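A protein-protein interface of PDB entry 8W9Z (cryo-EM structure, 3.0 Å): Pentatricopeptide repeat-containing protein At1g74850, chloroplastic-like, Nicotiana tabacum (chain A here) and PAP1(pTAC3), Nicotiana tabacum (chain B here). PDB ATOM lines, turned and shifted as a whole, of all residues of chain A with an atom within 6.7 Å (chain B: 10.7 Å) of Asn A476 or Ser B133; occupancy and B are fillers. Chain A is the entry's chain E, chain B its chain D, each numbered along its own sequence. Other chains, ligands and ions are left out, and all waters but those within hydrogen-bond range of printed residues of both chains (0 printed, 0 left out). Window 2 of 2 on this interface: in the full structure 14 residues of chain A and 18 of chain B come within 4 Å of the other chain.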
ATOM      1  N   GLU A 469      -2.641  30.456  18.856  1.00  0.00           N
ATOM      2  CA  GLU A 469      -2.559  30.287  17.410  1.00  0.00           C
ATOM      3  C   GLU A 469      -2.565  28.823  16.994  1.00  0.00           C
ATOM      4  O   GLU A 469      -3.090  28.490  15.925  1.00  0.00           O
ATOM      5  CB  GLU A 469      -1.312  30.982  16.864  1.00  0.00           C
ATOM      6  CG  GLU A 469      -1.507  32.463  16.597  1.00  0.00           C
ATOM      7  CD  GLU A 469      -2.431  32.730  15.421  1.00  0.00           C
ATOM      8  OE1 GLU A 469      -2.598  31.829  14.570  1.00  0.00           O
ATOM      9  OE2 GLU A 469      -2.991  33.843  15.347  1.00  0.00           O
ATOM     10  N   ALA A 471      -4.316  26.429  18.433  1.00  0.00           N
ATOM     11  CA  ALA A 471      -5.705  25.994  18.438  1.00  0.00           C
ATOM     12  C   ALA A 471      -6.443  26.493  17.203  1.00  0.00           C
ATOM     13  O   ALA A 471      -7.246  25.761  16.615  1.00  0.00           O
ATOM     14  CB  ALA A 471      -6.406  26.474  19.712  1.00  0.00           C
ATOM     15  N   VAL A 472      -6.164  27.731  16.790  1.00  0.00           N
ATOM     16  CA  VAL A 472      -6.766  28.263  15.572  1.00  0.00           C
ATOM     17  C   VAL A 472      -6.351  27.442  14.361  1.00  0.00           C
ATOM     18  O   VAL A 472      -7.193  27.079  13.530  1.00  0.00           O
ATOM     19  CB  VAL A 472      -6.398  29.749  15.404  1.00  0.00           C
ATOM     20  CG1 VAL A 472      -6.858  30.259  14.050  1.00  0.00           C
ATOM     21  CG2 VAL A 472      -7.018  30.574  16.518  1.00  0.00           C
ATOM     22  N   VAL A 473      -5.059  27.124  14.237  1.00  0.00           N
ATOM     23  CA  VAL A 473      -4.628  26.360  13.070  1.00  0.00           C
ATOM     24  C   VAL A 473      -5.116  24.917  13.132  1.00  0.00           C
ATOM     25  O   VAL A 473      -5.399  24.323  12.084  1.00  0.00           O
ATOM     26  CB  VAL A 473      -3.100  26.401  12.880  1.00  0.00           C
ATOM     27  CG1 VAL A 473      -2.597  27.838  12.871  1.00  0.00           C
ATOM     28  CG2 VAL A 473      -2.385  25.587  13.940  1.00  0.00           C
ATOM     29  N   ALA A 474      -5.258  24.343  14.328  1.00  0.00           N
ATOM     30  CA  ALA A 474      -5.829  23.008  14.433  1.00  0.00           C
ATOM     31  C   ALA A 474      -7.300  22.998  14.045  1.00  0.00           C
ATOM     32  O   ALA A 474      -7.754  22.065  13.374  1.00  0.00           O
ATOM     33  CB  ALA A 474      -5.645  22.467  15.851  1.00  0.00           C
ATOM     34  N   PHE A 475      -8.051  24.032  14.428  1.00  0.00           N
ATOM     35  CA  PHE A 475      -9.435  24.138  13.988  1.00  0.00           C
ATOM     36  C   PHE A 475      -9.528  24.354  12.485  1.00  0.00           C
ATOM     37  O   PHE A 475     -10.433  23.815  11.838  1.00  0.00           O
ATOM     38  CB  PHE A 475     -10.143  25.271  14.733  1.00  0.00           C
ATOM     39  CG  PHE A 475     -11.595  25.411  14.383  1.00  0.00           C
ATOM     40  CD1 PHE A 475     -12.465  24.348  14.560  1.00  0.00           C
ATOM     41  CD2 PHE A 475     -12.092  26.603  13.884  1.00  0.00           C
ATOM     42  CE1 PHE A 475     -13.804  24.469  14.240  1.00  0.00           C
ATOM     43  CE2 PHE A 475     -13.431  26.732  13.565  1.00  0.00           C
ATOM     44  CZ  PHE A 475     -14.286  25.661  13.740  1.00  0.00           C
ATOM     45  N   ASN A 476      -8.595  25.115  11.909  1.00  0.00           N
ATOM     46  CA  ASN A 476      -8.570  25.274  10.458  1.00  0.00           C
ATOM     47  C   ASN A 476      -8.304  23.945   9.761  1.00  0.00           C
ATOM     48  O   ASN A 476      -8.967  23.613   8.770  1.00  0.00           O
ATOM     49  CB  ASN A 476      -7.521  26.311  10.061  1.00  0.00           C
ATOM     50  CG  ASN A 476      -7.921  27.716  10.448  1.00  0.00           C
ATOM     51  OD1 ASN A 476      -7.150  28.447  11.067  1.00  0.00           O
ATOM     52  ND2 ASN A 476      -9.141  28.102  10.090  1.00  0.00           N
ATOM     53  N   THR A 477      -7.341  23.169  10.265  1.00  0.00           N
ATOM     54  CA  THR A 477      -7.080  21.856   9.687  1.00  0.00           C
ATOM     55  C   THR A 477      -8.290  20.943   9.835  1.00  0.00           C
ATOM     56  O   THR A 477      -8.584  20.143   8.940  1.00  0.00           O
ATOM     57  CB  THR A 477      -5.850  21.220  10.336  1.00  0.00           C
ATOM     58  OG1 THR A 477      -6.009  21.214  11.760  1.00  0.00           O
ATOM     59  CG2 THR A 477      -4.591  21.987   9.964  1.00  0.00           C
ATOM     60  N   MET A 478      -8.999  21.047  10.961  1.00  0.00           N
ATOM     61  CA  MET A 478     -10.232  20.289  11.136  1.00  0.00           C
ATOM     62  C   MET A 478     -11.270  20.684  10.094  1.00  0.00           C
ATOM     63  O   MET A 478     -11.992  19.830   9.567  1.00  0.00           O
ATOM     64  CB  MET A 478     -10.780  20.502  12.547  1.00  0.00           C
ATOM     65  CG  MET A 478     -12.007  19.667  12.861  1.00  0.00           C
ATOM     66  SD  MET A 478     -12.754  20.090  14.445  1.00  0.00           S
ATOM     67  CE  MET A 478     -14.060  18.869  14.524  1.00  0.00           C
ATOM     68  N   ASN A 479     -11.361  21.978   9.784  1.00  0.00           N
ATOM     69  CA  ASN A 479     -12.291  22.477   8.777  1.00  0.00           C
ATOM     70  C   ASN A 479     -11.792  22.221   7.359  1.00  0.00           C
ATOM     71  O   ASN A 479     -12.527  22.444   6.391  1.00  0.00           O
ATOM     72  CB  ASN A 479     -12.537  23.973   8.969  1.00  0.00           C
ATOM     73  CG  ASN A 479     -12.929  24.330  10.385  1.00  0.00           C
ATOM     74  OD1 ASN A 479     -13.597  23.560  11.072  1.00  0.00           O
ATOM     75  ND2 ASN A 479     -12.514  25.512  10.826  1.00  0.00           N
ATOM     76  N   GLU A 480     -10.559  21.735   7.218  1.00  0.00           N
ATOM     77  CA  GLU A 480      -9.971  21.551   5.897  1.00  0.00           C
ATOM     78  C   GLU A 480      -9.486  20.120   5.712  1.00  0.00           C
ATOM     79  O   GLU A 480      -8.567  19.865   4.927  1.00  0.00           O
ATOM     80  CB  GLU A 480      -8.819  22.535   5.688  1.00  0.00           C
ATOM     81  CG  GLU A 480      -8.737  23.103   4.283  1.00  0.00           C
ATOM     82  CD  GLU A 480      -9.772  24.183   4.037  1.00  0.00           C
ATOM     83  OE1 GLU A 480      -9.947  25.046   4.922  1.00  0.00           O
ATOM     84  OE2 GLU A 480     -10.413  24.166   2.966  1.00  0.00           O
ATOM     85  N   VAL A 481     -10.092  19.183   6.435  1.00  0.00           N
ATOM     86  CA  VAL A 481      -9.720  17.779   6.331  1.00  0.00           C
ATOM     87  C   VAL A 481     -10.878  16.888   5.897  1.00  0.00           C
ATOM     88  O   VAL A 481     -10.631  15.794   5.362  1.00  0.00           O
ATOM     89  CB  VAL A 481      -9.115  17.266   7.658  1.00  0.00           C
ATOM     90  CG1 VAL A 481     -10.199  17.061   8.712  1.00  0.00           C
ATOM     91  CG2 VAL A 481      -8.306  15.993   7.434  1.00  0.00           C
ATOM     92  N   SER B 102       4.063  41.807  16.192  1.00  0.00           N
ATOM     93  CA  SER B 102       3.471  40.749  15.390  1.00  0.00           C
ATOM     94  C   SER B 102       4.524  40.143  14.465  1.00  0.00           C
ATOM     95  O   SER B 102       5.391  40.860  13.955  1.00  0.00           O
ATOM     96  CB  SER B 102       2.301  41.292  14.569  1.00  0.00           C
ATOM     97  OG  SER B 102       1.752  40.290  13.732  1.00  0.00           O
ATOM     98  N   PRO B 103       4.482  38.833  14.234  1.00  0.00           N
ATOM     99  CA  PRO B 103       5.475  38.214  13.352  1.00  0.00           C
ATOM    100  C   PRO B 103       5.259  38.614  11.902  1.00  0.00           C
ATOM    101  O   PRO B 103       4.133  38.839  11.453  1.00  0.00           O
ATOM    102  CB  PRO B 103       5.243  36.713  13.555  1.00  0.00           C
ATOM    103  CG  PRO B 103       3.813  36.616  13.969  1.00  0.00           C
ATOM    104  CD  PRO B 103       3.539  37.847  14.787  1.00  0.00           C
ATOM    105  N   PHE B 108       8.899  34.230   9.555  1.00  0.00           N
ATOM    106  CA  PHE B 108       8.367  32.907   9.253  1.00  0.00           C
ATOM    107  C   PHE B 108       9.154  32.202   8.158  1.00  0.00           C
ATOM    108  O   PHE B 108       9.098  30.970   8.067  1.00  0.00           O
ATOM    109  CB  PHE B 108       6.894  33.009   8.857  1.00  0.00           C
ATOM    110  CG  PHE B 108       5.967  33.199  10.021  1.00  0.00           C
ATOM    111  CD1 PHE B 108       6.298  32.709  11.273  1.00  0.00           C
ATOM    112  CD2 PHE B 108       4.764  33.865   9.865  1.00  0.00           C
ATOM    113  CE1 PHE B 108       5.447  32.880  12.348  1.00  0.00           C
ATOM    114  CE2 PHE B 108       3.908  34.039  10.935  1.00  0.00           C
ATOM    115  CZ  PHE B 108       4.250  33.545  12.178  1.00  0.00           C
ATOM    116  N   MET B 125       4.375  22.289   6.055  1.00  0.00           N
ATOM    117  CA  MET B 125       2.966  22.589   5.823  1.00  0.00           C
ATOM    118  C   MET B 125       2.337  23.254   7.041  1.00  0.00           C
ATOM    119  O   MET B 125       1.521  24.176   6.904  1.00  0.00           O
ATOM    120  CB  MET B 125       2.209  21.311   5.460  1.00  0.00           C
ATOM    121  CG  MET B 125       2.172  21.005   3.974  1.00  0.00           C
ATOM    122  SD  MET B 125       1.206  22.214   3.052  1.00  0.00           S
ATOM    123  CE  MET B 125       1.151  21.445   1.436  1.00  0.00           C
ATOM    124  N   HIS B 126       2.705  22.801   8.241  1.00  0.00           N
ATOM    125  CA  HIS B 126       2.185  23.421   9.455  1.00  0.00           C
ATOM    126  C   HIS B 126       2.647  24.866   9.571  1.00  0.00           C
ATOM    127  O   HIS B 126       1.867  25.746   9.950  1.00  0.00           O
ATOM    128  CB  HIS B 126       2.620  22.615  10.680  1.00  0.00           C
ATOM    129  CG  HIS B 126       1.914  23.002  11.942  1.00  0.00           C
ATOM    130  ND1 HIS B 126       2.281  22.518  13.179  1.00  0.00           N
ATOM    131  CD2 HIS B 126       0.857  23.821  12.158  1.00  0.00           C
ATOM    132  CE1 HIS B 126       1.485  23.026  14.103  1.00  0.00           C
ATOM    133  NE2 HIS B 126       0.612  23.819  13.509  1.00  0.00           N
ATOM    134  N   ALA B 127       3.912  25.134   9.237  1.00  0.00           N
ATOM    135  CA  ALA B 127       4.412  26.505   9.264  1.00  0.00           C
ATOM    136  C   ALA B 127       3.707  27.371   8.227  1.00  0.00           C
ATOM    137  O   ALA B 127       3.407  28.543   8.488  1.00  0.00           O
ATOM    138  CB  ALA B 127       5.922  26.515   9.032  1.00  0.00           C
ATOM    139  N   LEU B 128       3.439  26.814   7.046  1.00  0.00           N
ATOM    140  CA  LEU B 128       2.718  27.561   6.019  1.00  0.00           C
ATOM    141  C   LEU B 128       1.309  27.909   6.486  1.00  0.00           C
ATOM    142  O   LEU B 128       0.840  29.037   6.296  1.00  0.00           O
ATOM    143  CB  LEU B 128       2.672  26.756   4.719  1.00  0.00           C
ATOM    144  CG  LEU B 128       1.872  27.384   3.577  1.00  0.00           C
ATOM    145  CD1 LEU B 128       2.471  28.723   3.177  1.00  0.00           C
ATOM    146  CD2 LEU B 128       1.800  26.443   2.384  1.00  0.00           C
ATOM    147  N   ARG B 129       0.620  26.945   7.099  1.00  0.00           N
ATOM    148  CA  ARG B 129      -0.719  27.213   7.616  1.00  0.00           C
ATOM    149  C   ARG B 129      -0.678  28.234   8.745  1.00  0.00           C
ATOM    150  O   ARG B 129      -1.572  29.081   8.859  1.00  0.00           O
ATOM    151  CB  ARG B 129      -1.372  25.913   8.085  1.00  0.00           C
ATOM    152  CG  ARG B 129      -1.873  25.039   6.949  1.00  0.00           C
ATOM    153  CD  ARG B 129      -2.526  23.771   7.465  1.00  0.00           C
ATOM    154  NE  ARG B 129      -1.552  22.856   8.051  1.00  0.00           N
ATOM    155  CZ  ARG B 129      -0.930  21.897   7.374  1.00  0.00           C
ATOM    156  NH1 ARG B 129      -1.180  21.725   6.083  1.00  0.00           N
ATOM    157  NH2 ARG B 129      -0.058  21.108   7.987  1.00  0.00           N
ATOM    158  N   ARG B 130       0.357  28.174   9.587  1.00  0.00           N
ATOM    159  CA  ARG B 130       0.517  29.163  10.647  1.00  0.00           C
ATOM    160  C   ARG B 130       0.677  30.562  10.068  1.00  0.00           C
ATOM    161  O   ARG B 130       0.036  31.515  10.525  1.00  0.00           O
ATOM    162  CB  ARG B 130       1.722  28.803  11.519  1.00  0.00           C
ATOM    163  CG  ARG B 130       2.127  29.889  12.500  1.00  0.00           C
ATOM    164  CD  ARG B 130       1.700  29.549  13.916  1.00  0.00           C
ATOM    165  NE  ARG B 130       2.369  28.351  14.412  1.00  0.00           N
ATOM    166  CZ  ARG B 130       2.232  27.875  15.645  1.00  0.00           C
ATOM    167  NH1 ARG B 130       1.449  28.498  16.514  1.00  0.00           N
ATOM    168  NH2 ARG B 130       2.879  26.777  16.010  1.00  0.00           N
ATOM    169  N   GLU B 131       1.533  30.702   9.054  1.00  0.00           N
ATOM    170  CA  GLU B 131       1.750  32.009   8.442  1.00  0.00           C
ATOM    171  C   GLU B 131       0.494  32.507   7.736  1.00  0.00           C
ATOM    172  O   GLU B 131       0.194  33.707   7.759  1.00  0.00           O
ATOM    173  CB  GLU B 131       2.926  31.940   7.468  1.00  0.00           C
ATOM    174  CG  GLU B 131       3.245  33.259   6.780  1.00  0.00           C
ATOM    175  CD  GLU B 131       4.500  33.184   5.933  1.00  0.00           C
ATOM    176  OE1 GLU B 131       5.040  32.070   5.764  1.00  0.00           O
ATOM    177  OE2 GLU B 131       4.949  34.240   5.439  1.00  0.00           O
ATOM    178  N   LEU B 132      -0.257  31.601   7.107  1.00  0.00           N
ATOM    179  CA  LEU B 132      -1.441  32.017   6.363  1.00  0.00           C
ATOM    180  C   LEU B 132      -2.609  32.345   7.287  1.00  0.00           C
ATOM    181  O   LEU B 132      -3.478  33.144   6.921  1.00  0.00           O
ATOM    182  CB  LEU B 132      -1.840  30.927   5.367  1.00  0.00           C
ATOM    183  CG  LEU B 132      -3.000  31.229   4.415  1.00  0.00           C
ATOM    184  CD1 LEU B 132      -2.692  32.451   3.563  1.00  0.00           C
ATOM    185  CD2 LEU B 132      -3.306  30.024   3.541  1.00  0.00           C
ATOM    186  N   SER B 133      -2.645  31.748   8.482  1.00  0.00           N
ATOM    187  CA  SER B 133      -3.781  31.949   9.376  1.00  0.00           C
ATOM    188  C   SER B 133      -3.890  33.393   9.851  1.00  0.00           C
ATOM    189  O   SER B 133      -5.004  33.896  10.039  1.00  0.00           O
ATOM    190  CB  SER B 133      -3.676  31.007  10.575  1.00  0.00           C
ATOM    191  OG  SER B 133      -3.685  29.651  10.160  1.00  0.00           O
ATOM    192  N   GLU B 134      -2.763  34.074  10.046  1.00  0.00           N
ATOM    193  CA  GLU B 134      -2.765  35.447  10.537  1.00  0.00           C
ATOM    194  C   GLU B 134      -3.061  36.473   9.449  1.00  0.00           C
ATOM    195  O   GLU B 134      -2.844  37.668   9.674  1.00  0.00           O
ATOM    196  CB  GLU B 134      -1.425  35.772  11.203  1.00  0.00           C
ATOM    197  CG  GLU B 134      -1.148  34.971  12.462  1.00  0.00           C
ATOM    198  CD  GLU B 134      -0.004  33.996  12.291  1.00  0.00           C
ATOM    199  OE1 GLU B 134       0.764  34.146  11.318  1.00  0.00           O
ATOM    200  OE2 GLU B 134       0.127  33.077  13.127  1.00  0.00           O
ATOM    201  N   GLY B 135      -3.550  36.043   8.290  1.00  0.00           N
ATOM    202  CA  GLY B 135      -3.866  36.972   7.219  1.00  0.00           C
ATOM    203  C   GLY B 135      -2.659  37.653   6.612  1.00  0.00           C
ATOM    204  O   GLY B 135      -2.704  38.861   6.342  1.00  0.00           O
ATOM    205  N   LEU B 136      -1.579  36.909   6.389  1.00  0.00           N
ATOM    206  CA  LEU B 136      -0.362  37.444   5.796  1.00  0.00           C
ATOM    207  C   LEU B 136       0.075  36.520   4.670  1.00  0.00           C
ATOM    208  O   LEU B 136       0.258  35.317   4.885  1.00  0.00           O
ATOM    209  CB  LEU B 136       0.751  37.582   6.842  1.00  0.00           C
ATOM    210  CG  LEU B 136       1.726  38.757   6.718  1.00  0.00           C
ATOM    211  CD1 LEU B 136       2.650  38.806   7.925  1.00  0.00           C
ATOM    212  CD2 LEU B 136       2.537  38.688   5.431  1.00  0.00           C
ATOM    213  N   ARG B 137       0.239  37.080   3.479  1.00  0.00           N
ATOM    214  CA  ARG B 137       0.626  36.281   2.322  1.00  0.00           C
ATOM    215  C   ARG B 137       2.112  35.946   2.393  1.00  0.00           C
ATOM    216  O   ARG B 137       2.932  36.838   2.631  1.00  0.00           O
ATOM    217  CB  ARG B 137       0.306  37.026   1.029  1.00  0.00           C
ATOM    218  CG  ARG B 137       0.782  38.472   1.002  1.00  0.00           C
ATOM    219  CD  ARG B 137       0.030  39.284  -0.040  1.00  0.00           C
ATOM    220  NE  ARG B 137       0.166  38.727  -1.382  1.00  0.00           N
ATOM    221  CZ  ARG B 137       1.094  39.103  -2.254  1.00  0.00           C
ATOM    222  NH1 ARG B 137       1.974  40.040  -1.928  1.00  0.00           N
ATOM    223  NH2 ARG B 137       1.142  38.545  -3.456  1.00  0.00           N
ATOM    224  N   PRO B 138       2.492  34.685   2.209  1.00  0.00           N
ATOM    225  CA  PRO B 138       3.909  34.321   2.298  1.00  0.00           C
ATOM    226  C   PRO B 138       4.711  34.900   1.145  1.00  0.00           C
ATOM    227  O   PRO B 138       4.171  35.366   0.139  1.00  0.00           O
ATOM    228  CB  PRO B 138       3.889  32.787   2.243  1.00  0.00           C
ATOM    229  CG  PRO B 138       2.480  32.401   2.576  1.00  0.00           C
ATOM    230  CD  PRO B 138       1.629  33.507   2.039  1.00  0.00           C
ATOM    231  N   PHE B 143       7.574  29.798  -0.791  1.00  0.00           N
ATOM    232  CA  PHE B 143       6.851  28.927  -1.711  1.00  0.00           C
ATOM    233  C   PHE B 143       7.807  28.172  -2.623  1.00  0.00           C
ATOM    234  O   PHE B 143       7.573  27.003  -2.949  1.00  0.00           O
ATOM    235  CB  PHE B 143       5.854  29.745  -2.530  1.00  0.00           C
ATOM    236  CG  PHE B 143       4.548  29.984  -1.830  1.00  0.00           C
ATOM    237  CD1 PHE B 143       3.993  29.006  -1.026  1.00  0.00           C
ATOM    238  CD2 PHE B 143       3.879  31.186  -1.975  1.00  0.00           C
ATOM    239  CE1 PHE B 143       2.791  29.220  -0.381  1.00  0.00           C
ATOM    240  CE2 PHE B 143       2.678  31.406  -1.332  1.00  0.00           C
ATOM    241  CZ  PHE B 143       2.134  30.423  -0.534  1.00  0.00           C
ATOM    242  N   LYS B 168      -3.260  32.084  -6.874  1.00  0.00           N
ATOM    243  CA  LYS B 168      -4.335  32.864  -6.272  1.00  0.00           C
ATOM    244  C   LYS B 168      -3.812  34.070  -5.503  1.00  0.00           C
ATOM    245  O   LYS B 168      -4.590  34.981  -5.202  1.00  0.00           O
ATOM    246  CB  LYS B 168      -5.185  31.985  -5.351  1.00  0.00           C
ATOM    247  CG  LYS B 168      -4.520  31.621  -4.035  1.00  0.00           C
ATOM    248  CD  LYS B 168      -5.459  30.824  -3.141  1.00  0.00           C
ATOM    249  CE  LYS B 168      -4.805  30.499  -1.807  1.00  0.00           C
ATOM    250  NZ  LYS B 168      -5.727  29.760  -0.898  1.00  0.00           N
ATOM    251  N   LEU B 169      -2.520  34.098  -5.179  1.00  0.00           N
ATOM    252  CA  LEU B 169      -1.898  35.239  -4.522  1.00  0.00           C
ATOM    253  C   LEU B 169      -1.268  36.213  -5.512  1.00  0.00           C
ATOM    254  O   LEU B 169      -0.414  37.017  -5.118  1.00  0.00           O
ATOM    255  CB  LEU B 169      -0.851  34.761  -3.515  1.00  0.00           C
ATOM    256  CG  LEU B 169      -1.387  34.007  -2.299  1.00  0.00           C
ATOM    257  CD1 LEU B 169      -0.251  33.608  -1.371  1.00  0.00           C
ATOM    258  CD2 LEU B 169      -2.418  34.845  -1.559  1.00  0.00           C
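Among the printed residues, pairs that only touch across the chains: Val A473 with Ser B133, Val A473 with His B126, Thr A477 with Arg B129, Glu A469 with Arg B130 and Asn A476 with Ser B133.
O of Arg B129 sits at hydrogen-bond distance from OG of Ser B133, at 2.5 Å. The side-chain amide oxygen (OD1) of Asn A476 lies close to the backbone carbonyl oxygen (O) of Val A472. OG1 of Thr A477 lies within hydrogen-bond range of O of Val A473 (3.2 Å). O of Ala A474 is in hydrogen-bond range of OG1 of Thr A477.
Of the printed residues of chain B, Glu A469 touches Arg B130 and Glu B134. No residue of chain B comes within 4 Å of Val A472. No residue of chain B comes within 4 Å of Ala A474. Of chain B, only Ser B133 (3.8 Å) comes within 4 Å of Asn A476. Thr A477 touches one residue of chain B. No residue of chain B comes within 4 Å of Asn A479. Met B125 touches none of the printed residues of chain A. Of the printed residues of chain A, His B126 touches Val A473 (3.5 Å). Of chain A, only Val A473 and Asn A476 come within 4 Å of Ser B133. Of the printed residues of chain A, Glu B134 touches Glu A469 (3.3 Å). The nearest residue of chain B that does not touch Asn A476 is Arg B129 (6.0 Å).
The side-chain carboxylate (OE1) of Glu A469 lies close to the side-chain carboxylate (OE2) of Glu B134 (3.3 Å).
Of the 12 printed residues of chain A, 4 touch a printed residue of chain B. Printed residues of chain A that touch a printed residue of chain B: Glu A469, Val A473, Asn A476 and Thr A477. Hydrophobic or aromatic side chains of chain A that line the printed part of chain B: Val A473. Printed residues of chain B that touch a printed residue of chain A: His B126, Arg B129, Arg B130, Ser B133 and Glu B134. Along chain B the printed residues that touch a printed residue of chain A span positions 126 to 134. Among the printed residues, 6 pairs touch across the chains.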
